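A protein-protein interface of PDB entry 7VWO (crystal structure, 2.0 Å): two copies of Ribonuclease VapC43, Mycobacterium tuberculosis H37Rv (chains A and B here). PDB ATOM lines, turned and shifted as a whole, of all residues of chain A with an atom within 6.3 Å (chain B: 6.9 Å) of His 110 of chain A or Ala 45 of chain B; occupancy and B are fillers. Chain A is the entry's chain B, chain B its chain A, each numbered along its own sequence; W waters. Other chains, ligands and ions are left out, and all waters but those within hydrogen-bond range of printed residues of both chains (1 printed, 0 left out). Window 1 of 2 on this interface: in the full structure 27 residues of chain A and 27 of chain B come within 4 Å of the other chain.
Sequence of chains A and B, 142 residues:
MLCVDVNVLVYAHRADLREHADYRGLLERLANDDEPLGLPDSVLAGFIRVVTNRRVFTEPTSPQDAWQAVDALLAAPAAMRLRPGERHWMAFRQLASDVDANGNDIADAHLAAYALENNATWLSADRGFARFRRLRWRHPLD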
ATOM      1  N   SER A  42      20.835  33.427  -7.088  1.00  0.00           N
ATOM      2  CA  SER A  42      22.073  33.469  -6.257  1.00  0.00           C
ATOM      3  C   SER A  42      23.071  34.490  -6.840  1.00  0.00           C
ATOM      4  O   SER A  42      23.811  35.090  -6.049  1.00  0.00           O
ATOM      5  CB  SER A  42      22.694  32.087  -6.134  1.00  0.00           C
ATOM      6  OG  SER A  42      23.090  31.597  -7.403  1.00  0.00           O
ATOM      7  N   PRO A  84      16.522  27.591  -9.135  1.00  0.00           N
ATOM      8  CA  PRO A  84      17.028  26.256  -9.376  1.00  0.00           C
ATOM      9  C   PRO A  84      15.852  25.381  -9.856  1.00  0.00           C
ATOM     10  O   PRO A  84      14.808  25.456  -9.290  1.00  0.00           O
ATOM     11  CB  PRO A  84      17.491  25.805  -7.991  1.00  0.00           C
ATOM     12  CG  PRO A  84      17.768  27.101  -7.248  1.00  0.00           C
ATOM     13  CD  PRO A  84      16.736  28.076  -7.776  1.00  0.00           C
ATOM     14  N   HIS A  88      18.485  20.778 -10.582  1.00  0.00           N
ATOM     15  CA  HIS A  88      19.640  21.601 -10.116  1.00  0.00           C
ATOM     16  C   HIS A  88      20.425  20.872  -9.015  1.00  0.00           C
ATOM     17  O   HIS A  88      21.646  20.836  -9.119  1.00  0.00           O
ATOM     18  CB  HIS A  88      19.144  22.956  -9.593  1.00  0.00           C
ATOM     19  CG  HIS A  88      20.256  23.919  -9.331  1.00  0.00           C
ATOM     20  ND1 HIS A  88      21.004  23.882  -8.172  1.00  0.00           N
ATOM     21  CD2 HIS A  88      20.762  24.930 -10.072  1.00  0.00           C
ATOM     22  CE1 HIS A  88      21.911  24.840  -8.203  1.00  0.00           C
ATOM     23  NE2 HIS A  88      21.786  25.494  -9.358  1.00  0.00           N
ATOM     24  N   TRP A  89      19.737  20.256  -8.053  1.00  0.00           N
ATOM     25  CA  TRP A  89      20.457  19.633  -6.913  1.00  0.00           C
ATOM     26  C   TRP A  89      21.369  18.483  -7.392  1.00  0.00           C
ATOM     27  O   TRP A  89      22.516  18.423  -6.971  1.00  0.00           O
ATOM     28  CB  TRP A  89      19.439  19.144  -5.878  1.00  0.00           C
ATOM     29  CG  TRP A  89      20.007  18.476  -4.665  1.00  0.00           C
ATOM     30  CD1 TRP A  89      19.919  17.154  -4.341  1.00  0.00           C
ATOM     31  CD2 TRP A  89      20.700  19.108  -3.575  1.00  0.00           C
ATOM     32  NE1 TRP A  89      20.528  16.917  -3.140  1.00  0.00           N
ATOM     33  CE2 TRP A  89      21.008  18.097  -2.641  1.00  0.00           C
ATOM     34  CE3 TRP A  89      21.099  20.421  -3.305  1.00  0.00           C
ATOM     35  CZ2 TRP A  89      21.711  18.359  -1.466  1.00  0.00           C
ATOM     36  CZ3 TRP A  89      21.782  20.679  -2.136  1.00  0.00           C
ATOM     37  CH2 TRP A  89      22.083  19.661  -1.233  1.00  0.00           C
ATOM     38  N   PHE A  92      24.320  19.886  -9.294  1.00  0.00           N
ATOM     39  CA  PHE A  92      25.308  20.450  -8.335  1.00  0.00           C
ATOM     40  C   PHE A  92      26.154  19.304  -7.741  1.00  0.00           C
ATOM     41  O   PHE A  92      27.382  19.403  -7.705  1.00  0.00           O
ATOM     42  CB  PHE A  92      24.544  21.221  -7.261  1.00  0.00           C
ATOM     43  CG  PHE A  92      25.261  21.438  -5.952  1.00  0.00           C
ATOM     44  CD1 PHE A  92      26.544  21.959  -5.918  1.00  0.00           C
ATOM     45  CD2 PHE A  92      24.640  21.142  -4.747  1.00  0.00           C
ATOM     46  CE1 PHE A  92      27.192  22.172  -4.712  1.00  0.00           C
ATOM     47  CE2 PHE A  92      25.293  21.343  -3.542  1.00  0.00           C
ATOM     48  CZ  PHE A  92      26.569  21.859  -3.525  1.00  0.00           C
ATOM     49  N   LEU A  95      28.632  17.925 -10.452  1.00  0.00           N
ATOM     50  CA  LEU A  95      29.781  18.849 -10.660  1.00  0.00           C
ATOM     51  C   LEU A  95      30.758  18.769  -9.472  1.00  0.00           C
ATOM     52  O   LEU A  95      31.976  18.692  -9.716  1.00  0.00           O
ATOM     53  CB  LEU A  95      29.222  20.261 -10.826  1.00  0.00           C
ATOM     54  CG  LEU A  95      28.536  20.556 -12.159  1.00  0.00           C
ATOM     55  CD1 LEU A  95      27.742  21.850 -12.085  1.00  0.00           C
ATOM     56  CD2 LEU A  95      29.556  20.617 -13.289  1.00  0.00           C
ATOM     57  N   ASP A 105      34.977  25.550  -3.780  1.00  0.00           N
ATOM     58  CA  ASP A 105      34.643  24.760  -4.988  1.00  0.00           C
ATOM     59  C   ASP A 105      33.134  24.466  -4.892  1.00  0.00           C
ATOM     60  O   ASP A 105      32.487  24.396  -5.928  1.00  0.00           O
ATOM     61  CB  ASP A 105      35.319  23.393  -5.023  1.00  0.00           C
ATOM     62  CG  ASP A 105      36.838  23.430  -5.101  1.00  0.00           C
ATOM     63  OD1 ASP A 105      37.379  24.455  -5.562  1.00  0.00           O
ATOM     64  OD2 ASP A 105      37.464  22.429  -4.704  1.00  0.00           O
ATOM     65  N   ILE A 106      32.645  24.234  -3.676  1.00  0.00           N
ATOM     66  CA  ILE A 106      31.207  23.898  -3.486  1.00  0.00           C
ATOM     67  C   ILE A 106      30.336  25.070  -3.971  1.00  0.00           C
ATOM     68  O   ILE A 106      29.364  24.817  -4.704  1.00  0.00           O
ATOM     69  CB  ILE A 106      30.959  23.601  -2.000  1.00  0.00           C
ATOM     70  CG1 ILE A 106      31.713  22.351  -1.541  1.00  0.00           C
ATOM     71  CG2 ILE A 106      29.466  23.493  -1.718  1.00  0.00           C
ATOM     72  CD1 ILE A 106      31.274  21.088  -2.230  1.00  0.00           C
ATOM     73  N   ALA A 107      30.723  26.297  -3.640  1.00  0.00           N
ATOM     74  CA  ALA A 107      29.977  27.498  -4.079  1.00  0.00           C
ATOM     75  C   ALA A 107      30.013  27.601  -5.608  1.00  0.00           C
ATOM     76  O   ALA A 107      28.941  27.808  -6.208  1.00  0.00           O
ATOM     77  CB  ALA A 107      30.586  28.719  -3.443  1.00  0.00           C
ATOM     78  N   ASP A 108      31.182  27.341  -6.199  1.00  0.00           N
ATOM     79  CA  ASP A 108      31.325  27.388  -7.677  1.00  0.00           C
ATOM     80  C   ASP A 108      30.422  26.314  -8.309  1.00  0.00           C
ATOM     81  O   ASP A 108      29.774  26.621  -9.301  1.00  0.00           O
ATOM     82  CB  ASP A 108      32.756  27.075  -8.102  1.00  0.00           C
ATOM     83  CG  ASP A 108      33.767  28.092  -7.587  1.00  0.00           C
ATOM     84  OD1 ASP A 108      33.346  29.190  -7.182  1.00  0.00           O
ATOM     85  OD2 ASP A 108      34.964  27.776  -7.592  1.00  0.00           O
ATOM     86  N   ALA A 109      30.419  25.126  -7.713  1.00  0.00           N
ATOM     87  CA  ALA A 109      29.633  23.997  -8.268  1.00  0.00           C
ATOM     88  C   ALA A 109      28.134  24.355  -8.220  1.00  0.00           C
ATOM     89  O   ALA A 109      27.435  24.158  -9.219  1.00  0.00           O
ATOM     90  CB  ALA A 109      29.966  22.748  -7.504  1.00  0.00           C
ATOM     91  N   HIS A 110      27.708  24.951  -7.113  1.00  0.00           N
ATOM     92  CA  HIS A 110      26.274  25.312  -6.959  1.00  0.00           C
ATOM     93  C   HIS A 110      25.889  26.334  -8.036  1.00  0.00           C
ATOM     94  O   HIS A 110      24.857  26.119  -8.687  1.00  0.00           O
ATOM     95  CB  HIS A 110      25.998  25.793  -5.525  1.00  0.00           C
ATOM     96  CG  HIS A 110      24.549  25.815  -5.173  1.00  0.00           C
ATOM     97  ND1 HIS A 110      23.739  26.891  -5.461  1.00  0.00           N
ATOM     98  CD2 HIS A 110      23.758  24.894  -4.578  1.00  0.00           C
ATOM     99  CE1 HIS A 110      22.513  26.643  -5.050  1.00  0.00           C
ATOM    100  NE2 HIS A 110      22.497  25.420  -4.506  1.00  0.00           N
ATOM    101  N   LEU A 111      26.732  27.346  -8.273  1.00  0.00           N
ATOM    102  CA  LEU A 111      26.490  28.350  -9.349  1.00  0.00           C
ATOM    103  C   LEU A 111      26.544  27.719 -10.746  1.00  0.00           C
ATOM    104  O   LEU A 111      25.596  27.928 -11.507  1.00  0.00           O
ATOM    105  CB  LEU A 111      27.568  29.435  -9.237  1.00  0.00           C
ATOM    106  CG  LEU A 111      27.354  30.443  -8.109  1.00  0.00           C
ATOM    107  CD1 LEU A 111      28.569  31.351  -7.954  1.00  0.00           C
ATOM    108  CD2 LEU A 111      26.103  31.266  -8.365  1.00  0.00           C
ATOM    109  N   ALA A 112      27.532  26.856 -10.980  1.00  0.00           N
ATOM    110  CA  ALA A 112      27.752  26.190 -12.290  1.00  0.00           C
ATOM    111  C   ALA A 112      26.531  25.312 -12.613  1.00  0.00           C
ATOM    112  O   ALA A 112      26.201  25.165 -13.796  1.00  0.00           O
ATOM    113  CB  ALA A 112      29.033  25.403 -12.251  1.00  0.00           C
ATOM    114  N   ALA A 113      25.922  24.763 -11.572  1.00  0.00           N
ATOM    115  CA  ALA A 113      24.742  23.880 -11.730  1.00  0.00           C
ATOM    116  C   ALA A 113      23.624  24.658 -12.454  1.00  0.00           C
ATOM    117  O   ALA A 113      22.894  24.001 -13.213  1.00  0.00           O
ATOM    118  CB  ALA A 113      24.289  23.389 -10.389  1.00  0.00           C
ATOM    119  N   TYR A 114      23.458  25.968 -12.222  1.00  0.00           N
ATOM    120  CA  TYR A 114      22.384  26.652 -12.994  1.00  0.00           C
ATOM    121  C   TYR A 114      22.657  26.534 -14.507  1.00  0.00           C
ATOM    122  O   TYR A 114      21.719  26.210 -15.260  1.00  0.00           O
ATOM    123  CB  TYR A 114      22.322  28.150 -12.682  1.00  0.00           C
ATOM    124  CG  TYR A 114      21.783  28.512 -11.322  1.00  0.00           C
ATOM    125  CD1 TYR A 114      20.461  28.886 -11.160  1.00  0.00           C
ATOM    126  CD2 TYR A 114      22.597  28.511 -10.201  1.00  0.00           C
ATOM    127  CE1 TYR A 114      19.953  29.231  -9.919  1.00  0.00           C
ATOM    128  CE2 TYR A 114      22.104  28.848  -8.951  1.00  0.00           C
ATOM    129  CZ  TYR A 114      20.777  29.214  -8.808  1.00  0.00           C
ATOM    130  OH  TYR A 114      20.279  29.552  -7.585  1.00  0.00           O
ATOM    131  N   VAL B   6      23.430  27.007   8.627  1.00  0.00           N
ATOM    132  CA  VAL B   6      24.693  26.242   8.414  1.00  0.00           C
ATOM    133  C   VAL B   6      25.337  25.929   9.768  1.00  0.00           C
ATOM    134  O   VAL B   6      25.708  24.760   9.978  1.00  0.00           O
ATOM    135  CB  VAL B   6      25.656  27.072   7.548  1.00  0.00           C
ATOM    136  CG1 VAL B   6      27.012  26.394   7.426  1.00  0.00           C
ATOM    137  CG2 VAL B   6      25.060  27.326   6.169  1.00  0.00           C
ATOM    138  N   PRO B  40      17.301  23.992   3.653  1.00  0.00           N
ATOM    139  CA  PRO B  40      17.441  24.707   2.410  1.00  0.00           C
ATOM    140  C   PRO B  40      18.647  24.113   1.647  1.00  0.00           C
ATOM    141  O   PRO B  40      19.615  23.745   2.269  1.00  0.00           O
ATOM    142  CB  PRO B  40      17.581  26.181   2.858  1.00  0.00           C
ATOM    143  CG  PRO B  40      17.059  26.207   4.273  1.00  0.00           C
ATOM    144  CD  PRO B  40      17.436  24.852   4.829  1.00  0.00           C
ATOM    145  N   ASP B  41      18.543  24.109   0.325  1.00  0.00           N
ATOM    146  CA  ASP B  41      19.670  23.593  -0.490  1.00  0.00           C
ATOM    147  C   ASP B  41      20.909  24.443  -0.167  1.00  0.00           C
ATOM    148  O   ASP B  41      21.963  23.871   0.030  1.00  0.00           O
ATOM    149  CB  ASP B  41      19.400  23.804  -1.968  1.00  0.00           C
ATOM    150  CG  ASP B  41      18.211  23.047  -2.530  1.00  0.00           C
ATOM    151  OD1 ASP B  41      17.789  22.071  -1.899  1.00  0.00           O
ATOM    152  OD2 ASP B  41      17.729  23.440  -3.607  1.00  0.00           O
ATOM    153  N   SER B  42      20.733  25.752  -0.038  1.00  0.00           N
ATOM    154  CA  SER B  42      21.854  26.696   0.256  1.00  0.00           C
ATOM    155  C   SER B  42      22.469  26.333   1.621  1.00  0.00           C
ATOM    156  O   SER B  42      23.686  26.504   1.772  1.00  0.00           O
ATOM    157  CB  SER B  42      21.388  28.148   0.187  1.00  0.00           C
ATOM    158  OG  SER B  42      20.333  28.400   1.095  1.00  0.00           O
ATOM    159  N   VAL B  43      21.634  25.956   2.598  1.00  0.00           N
ATOM    160  CA  VAL B  43      22.178  25.497   3.912  1.00  0.00           C
ATOM    161  C   VAL B  43      23.000  24.203   3.754  1.00  0.00           C
ATOM    162  O   VAL B  43      24.081  24.113   4.337  1.00  0.00           O
ATOM    163  CB  VAL B  43      21.063  25.318   4.956  1.00  0.00           C
ATOM    164  CG1 VAL B  43      21.472  24.432   6.118  1.00  0.00           C
ATOM    165  CG2 VAL B  43      20.558  26.666   5.455  1.00  0.00           C
ATOM    166  N   LEU B  44      22.468  23.241   2.997  1.00  0.00           N
ATOM    167  CA  LEU B  44      23.193  21.951   2.854  1.00  0.00           C
ATOM    168  C   LEU B  44      24.516  22.233   2.125  1.00  0.00           C
ATOM    169  O   LEU B  44      25.561  21.781   2.594  1.00  0.00           O
ATOM    170  CB  LEU B  44      22.280  21.000   2.077  1.00  0.00           C
ATOM    171  CG  LEU B  44      20.995  20.605   2.805  1.00  0.00           C
ATOM    172  CD1 LEU B  44      20.098  19.754   1.915  1.00  0.00           C
ATOM    173  CD2 LEU B  44      21.313  19.880   4.101  1.00  0.00           C
ATOM    174  N   ALA B  45      24.430  23.055   1.086  1.00  0.00           N
ATOM    175  CA  ALA B  45      25.625  23.413   0.293  1.00  0.00           C
ATOM    176  C   ALA B  45      26.611  24.195   1.207  1.00  0.00           C
ATOM    177  O   ALA B  45      27.797  23.875   1.183  1.00  0.00           O
ATOM    178  CB  ALA B  45      25.193  24.179  -0.915  1.00  0.00           C
ATOM    179  N   GLY B  46      26.088  25.107   2.040  1.00  0.00           N
ATOM    180  CA  GLY B  46      26.926  25.929   2.957  1.00  0.00           C
ATOM    181  C   GLY B  46      27.648  25.071   3.987  1.00  0.00           C
ATOM    182  O   GLY B  46      28.809  25.356   4.277  1.00  0.00           O
ATOM    183  N   PHE B  47      26.953  24.056   4.521  1.00  0.00           N
ATOM    184  CA  PHE B  47      27.574  23.133   5.495  1.00  0.00           C
ATOM    185  C   PHE B  47      28.755  22.382   4.845  1.00  0.00           C
ATOM    186  O   PHE B  47      29.825  22.316   5.443  1.00  0.00           O
ATOM    187  CB  PHE B  47      26.547  22.089   5.940  1.00  0.00           C
ATOM    188  CG  PHE B  47      27.093  20.843   6.587  1.00  0.00           C
ATOM    189  CD1 PHE B  47      27.504  20.851   7.908  1.00  0.00           C
ATOM    190  CD2 PHE B  47      27.165  19.653   5.881  1.00  0.00           C
ATOM    191  CE1 PHE B  47      27.991  19.702   8.505  1.00  0.00           C
ATOM    192  CE2 PHE B  47      27.658  18.503   6.476  1.00  0.00           C
ATOM    193  CZ  PHE B  47      28.066  18.530   7.789  1.00  0.00           C
ATOM    194  N   ILE B  48      28.547  21.901   3.616  1.00  0.00           N
ATOM    195  CA  ILE B  48      29.665  21.183   2.914  1.00  0.00           C
ATOM    196  C   ILE B  48      30.826  22.160   2.690  1.00  0.00           C
ATOM    197  O   ILE B  48      31.944  21.813   3.022  1.00  0.00           O
ATOM    198  CB  ILE B  48      29.216  20.575   1.578  1.00  0.00           C
ATOM    199  CG1 ILE B  48      27.960  19.715   1.736  1.00  0.00           C
ATOM    200  CG2 ILE B  48      30.351  19.783   0.947  1.00  0.00           C
ATOM    201  CD1 ILE B  48      27.498  19.082   0.451  1.00  0.00           C
ATOM    202  N   ARG B  49      30.503  23.372   2.259  1.00  0.00           N
ATOM    203  CA  ARG B  49      31.583  24.333   1.959  1.00  0.00           C
ATOM    204  C   ARG B  49      32.363  24.622   3.254  1.00  0.00           C
ATOM    205  O   ARG B  49      33.599  24.704   3.177  1.00  0.00           O
ATOM    206  CB  ARG B  49      30.933  25.595   1.396  1.00  0.00           C
ATOM    207  CG  ARG B  49      31.871  26.771   1.177  1.00  0.00           C
ATOM    208  CD  ARG B  49      31.243  27.678   0.139  1.00  0.00           C
ATOM    209  NE  ARG B  49      30.156  28.508   0.638  1.00  0.00           N
ATOM    210  CZ  ARG B  49      28.858  28.236   0.526  1.00  0.00           C
ATOM    211  NH1 ARG B  49      28.447  27.118  -0.052  1.00  0.00           N
ATOM    212  NH2 ARG B  49      27.968  29.088   1.003  1.00  0.00           N
ATOM    213  N   VAL B  50      31.652  24.834   4.372  1.00  0.00           N
ATOM    214  CA  VAL B  50      32.378  25.185   5.635  1.00  0.00           C
ATOM    215  C   VAL B  50      33.227  24.035   6.217  1.00  0.00           C
ATOM    216  O   VAL B  50      34.419  24.253   6.446  1.00  0.00           O
ATOM    217  CB  VAL B  50      31.388  25.695   6.704  1.00  0.00           C
ATOM    218  CG1 VAL B  50      32.024  25.818   8.079  1.00  0.00           C
ATOM    219  CG2 VAL B  50      30.701  26.986   6.286  1.00  0.00           C
ATOM    220  N   TRP B  67      29.386  14.832   2.258  1.00  0.00           N
ATOM    221  CA  TRP B  67      28.216  14.402   1.442  1.00  0.00           C
ATOM    222  C   TRP B  67      27.444  13.273   2.146  1.00  0.00           C
ATOM    223  O   TRP B  67      26.220  13.321   2.134  1.00  0.00           O
ATOM    224  CB  TRP B  67      28.617  14.070   0.000  1.00  0.00           C
ATOM    225  CG  TRP B  67      28.823  15.280  -0.855  1.00  0.00           C
ATOM    226  CD1 TRP B  67      30.011  15.781  -1.299  1.00  0.00           C
ATOM    227  CD2 TRP B  67      27.801  16.142  -1.387  1.00  0.00           C
ATOM    228  NE1 TRP B  67      29.801  16.891  -2.068  1.00  0.00           N
ATOM    229  CE2 TRP B  67      28.456  17.140  -2.141  1.00  0.00           C
ATOM    230  CE3 TRP B  67      26.405  16.173  -1.299  1.00  0.00           C
ATOM    231  CZ2 TRP B  67      27.761  18.151  -2.800  1.00  0.00           C
ATOM    232  CZ3 TRP B  67      25.718  17.167  -1.957  1.00  0.00           C
ATOM    233  CH2 TRP B  67      26.389  18.142  -2.697  1.00  0.00           C
ATOM    234  N   VAL B  70      25.272  14.743   4.822  1.00  0.00           N
ATOM    235  CA  VAL B  70      24.065  15.365   4.214  1.00  0.00           C
ATOM    236  C   VAL B  70      23.082  14.250   3.806  1.00  0.00           C
ATOM    237  O   VAL B  70      21.886  14.372   4.108  1.00  0.00           O
ATOM    238  CB  VAL B  70      24.455  16.240   3.007  1.00  0.00           C
ATOM    239  CG1 VAL B  70      23.276  16.573   2.109  1.00  0.00           C
ATOM    240  CG2 VAL B  70      25.192  17.500   3.447  1.00  0.00           C
ATOM    241  N   PRO B  84      14.372  26.997  -3.448  1.00  0.00           N
ATOM    242  CA  PRO B  84      13.697  28.280  -3.330  1.00  0.00           C
ATOM    243  C   PRO B  84      12.370  28.233  -4.097  1.00  0.00           C
ATOM    244  O   PRO B  84      12.358  27.827  -5.242  1.00  0.00           O
ATOM    245  CB  PRO B  84      14.695  29.229  -3.987  1.00  0.00           C
ATOM    246  CG  PRO B  84      16.038  28.564  -3.768  1.00  0.00           C
ATOM    247  CD  PRO B  84      15.753  27.084  -3.914  1.00  0.00           C
ATOM    248  N   TYR B 114      13.911  31.335   3.062  1.00  0.00           N
ATOM    249  CA  TYR B 114      13.323  29.974   3.088  1.00  0.00           C
ATOM    250  C   TYR B 114      12.337  29.825   4.270  1.00  0.00           C
ATOM    251  O   TYR B 114      11.237  29.271   4.056  1.00  0.00           O
ATOM    252  CB  TYR B 114      14.414  28.932   3.332  1.00  0.00           C
ATOM    253  CG  TYR B 114      15.352  28.704   2.174  1.00  0.00           C
ATOM    254  CD1 TYR B 114      15.070  27.756   1.203  1.00  0.00           C
ATOM    255  CD2 TYR B 114      16.527  29.427   2.049  1.00  0.00           C
ATOM    256  CE1 TYR B 114      15.927  27.533   0.137  1.00  0.00           C
ATOM    257  CE2 TYR B 114      17.396  29.217   0.991  1.00  0.00           C
ATOM    258  CZ  TYR B 114      17.097  28.263   0.032  1.00  0.00           C
ATOM    259  OH  TYR B 114      17.952  28.046  -1.009  1.00  0.00           O
HETATM  260  O   HOH W   1      20.189  23.152  -4.874  1.00  0.00           O
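NE2 of His 88 of chain A lies within hydrogen-bond range of O of His 110 of chain A, at 3.2 Å.
Among the printed residues, merely in contact across the chains: Pro 84 of chain A with Pro 84 of chain B, Trp 89 of chain A with Asp 41 of chain B, Trp 89 of chain A with Leu 44 of chain B, Phe 92 of chain A with Ala 45 of chain B, Phe 92 of chain A with Trp 67 of chain B, Ile 106 of chain A with Ala 45 of chain B, Ile 106 of chain A with Ile 48 of chain B, Ile 106 of chain A with Arg 49 of chain B, Ala 107 of chain A with Arg 49 of chain B and His 110 of chain A with Ala 45 of chain B.
Of the printed residues of chain B, His 110 of chain A touches Ala 45. Of the printed residues of chain A, Ala 45 of chain B touches Phe 92, Ile 106 and His 110. Of the printed residues of chain A, Pro 84 of chain B touches Pro 84. Of the printed residues of chain A, Trp 67 of chain B touches Phe 92. Leu 111 of chain A touches none of the printed residues of chain B. The nearest printed residue of chain B that does not touch His 110 of chain A is Asp 41 of chain B (4.3 Å). The nearest printed residue of chain B that does not touch Phe 92 of chain A is Ile 48 of chain B (4.9 Å).
Hydrophobic or aromatic side chains of chain A that line the printed part of chain B: Pro 84, Trp 89, Phe 92, Ile 106, Ala 107 and His 110. Along chain A the printed residues that touch a printed residue of chain B span positions 84 to 110. Of the 16 printed residues of chain B, 7 touch a printed residue of chain A. Printed residues of chain B that touch a printed residue of chain A: Asp 41, Leu 44, Ala 45, Ile 48, Arg 49, Trp 67 and Pro 84. Hydrophobic or aromatic side chains of chain B within 4 Å of the printed part of chain A: Leu 44, Ala 45, Ile 48, Trp 67 and Pro 84. Among the printed residues, no Asp or Glu carboxylate lies within 4 Å of a Lys or Arg side-chain nitrogen of the other chain.
Pro 84 of chain B touches its own counterpart, Pro 84 of chain A. Positions printed for both chains: 42, 84 and 114.
Water W1 lies within hydrogen-bond range of OD2 of Asp 41 of chain B (2.8 Å), NE2 of His 110 of chain A (3.3 Å) and ND1 of His 88 of chain A (3.5 Å).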
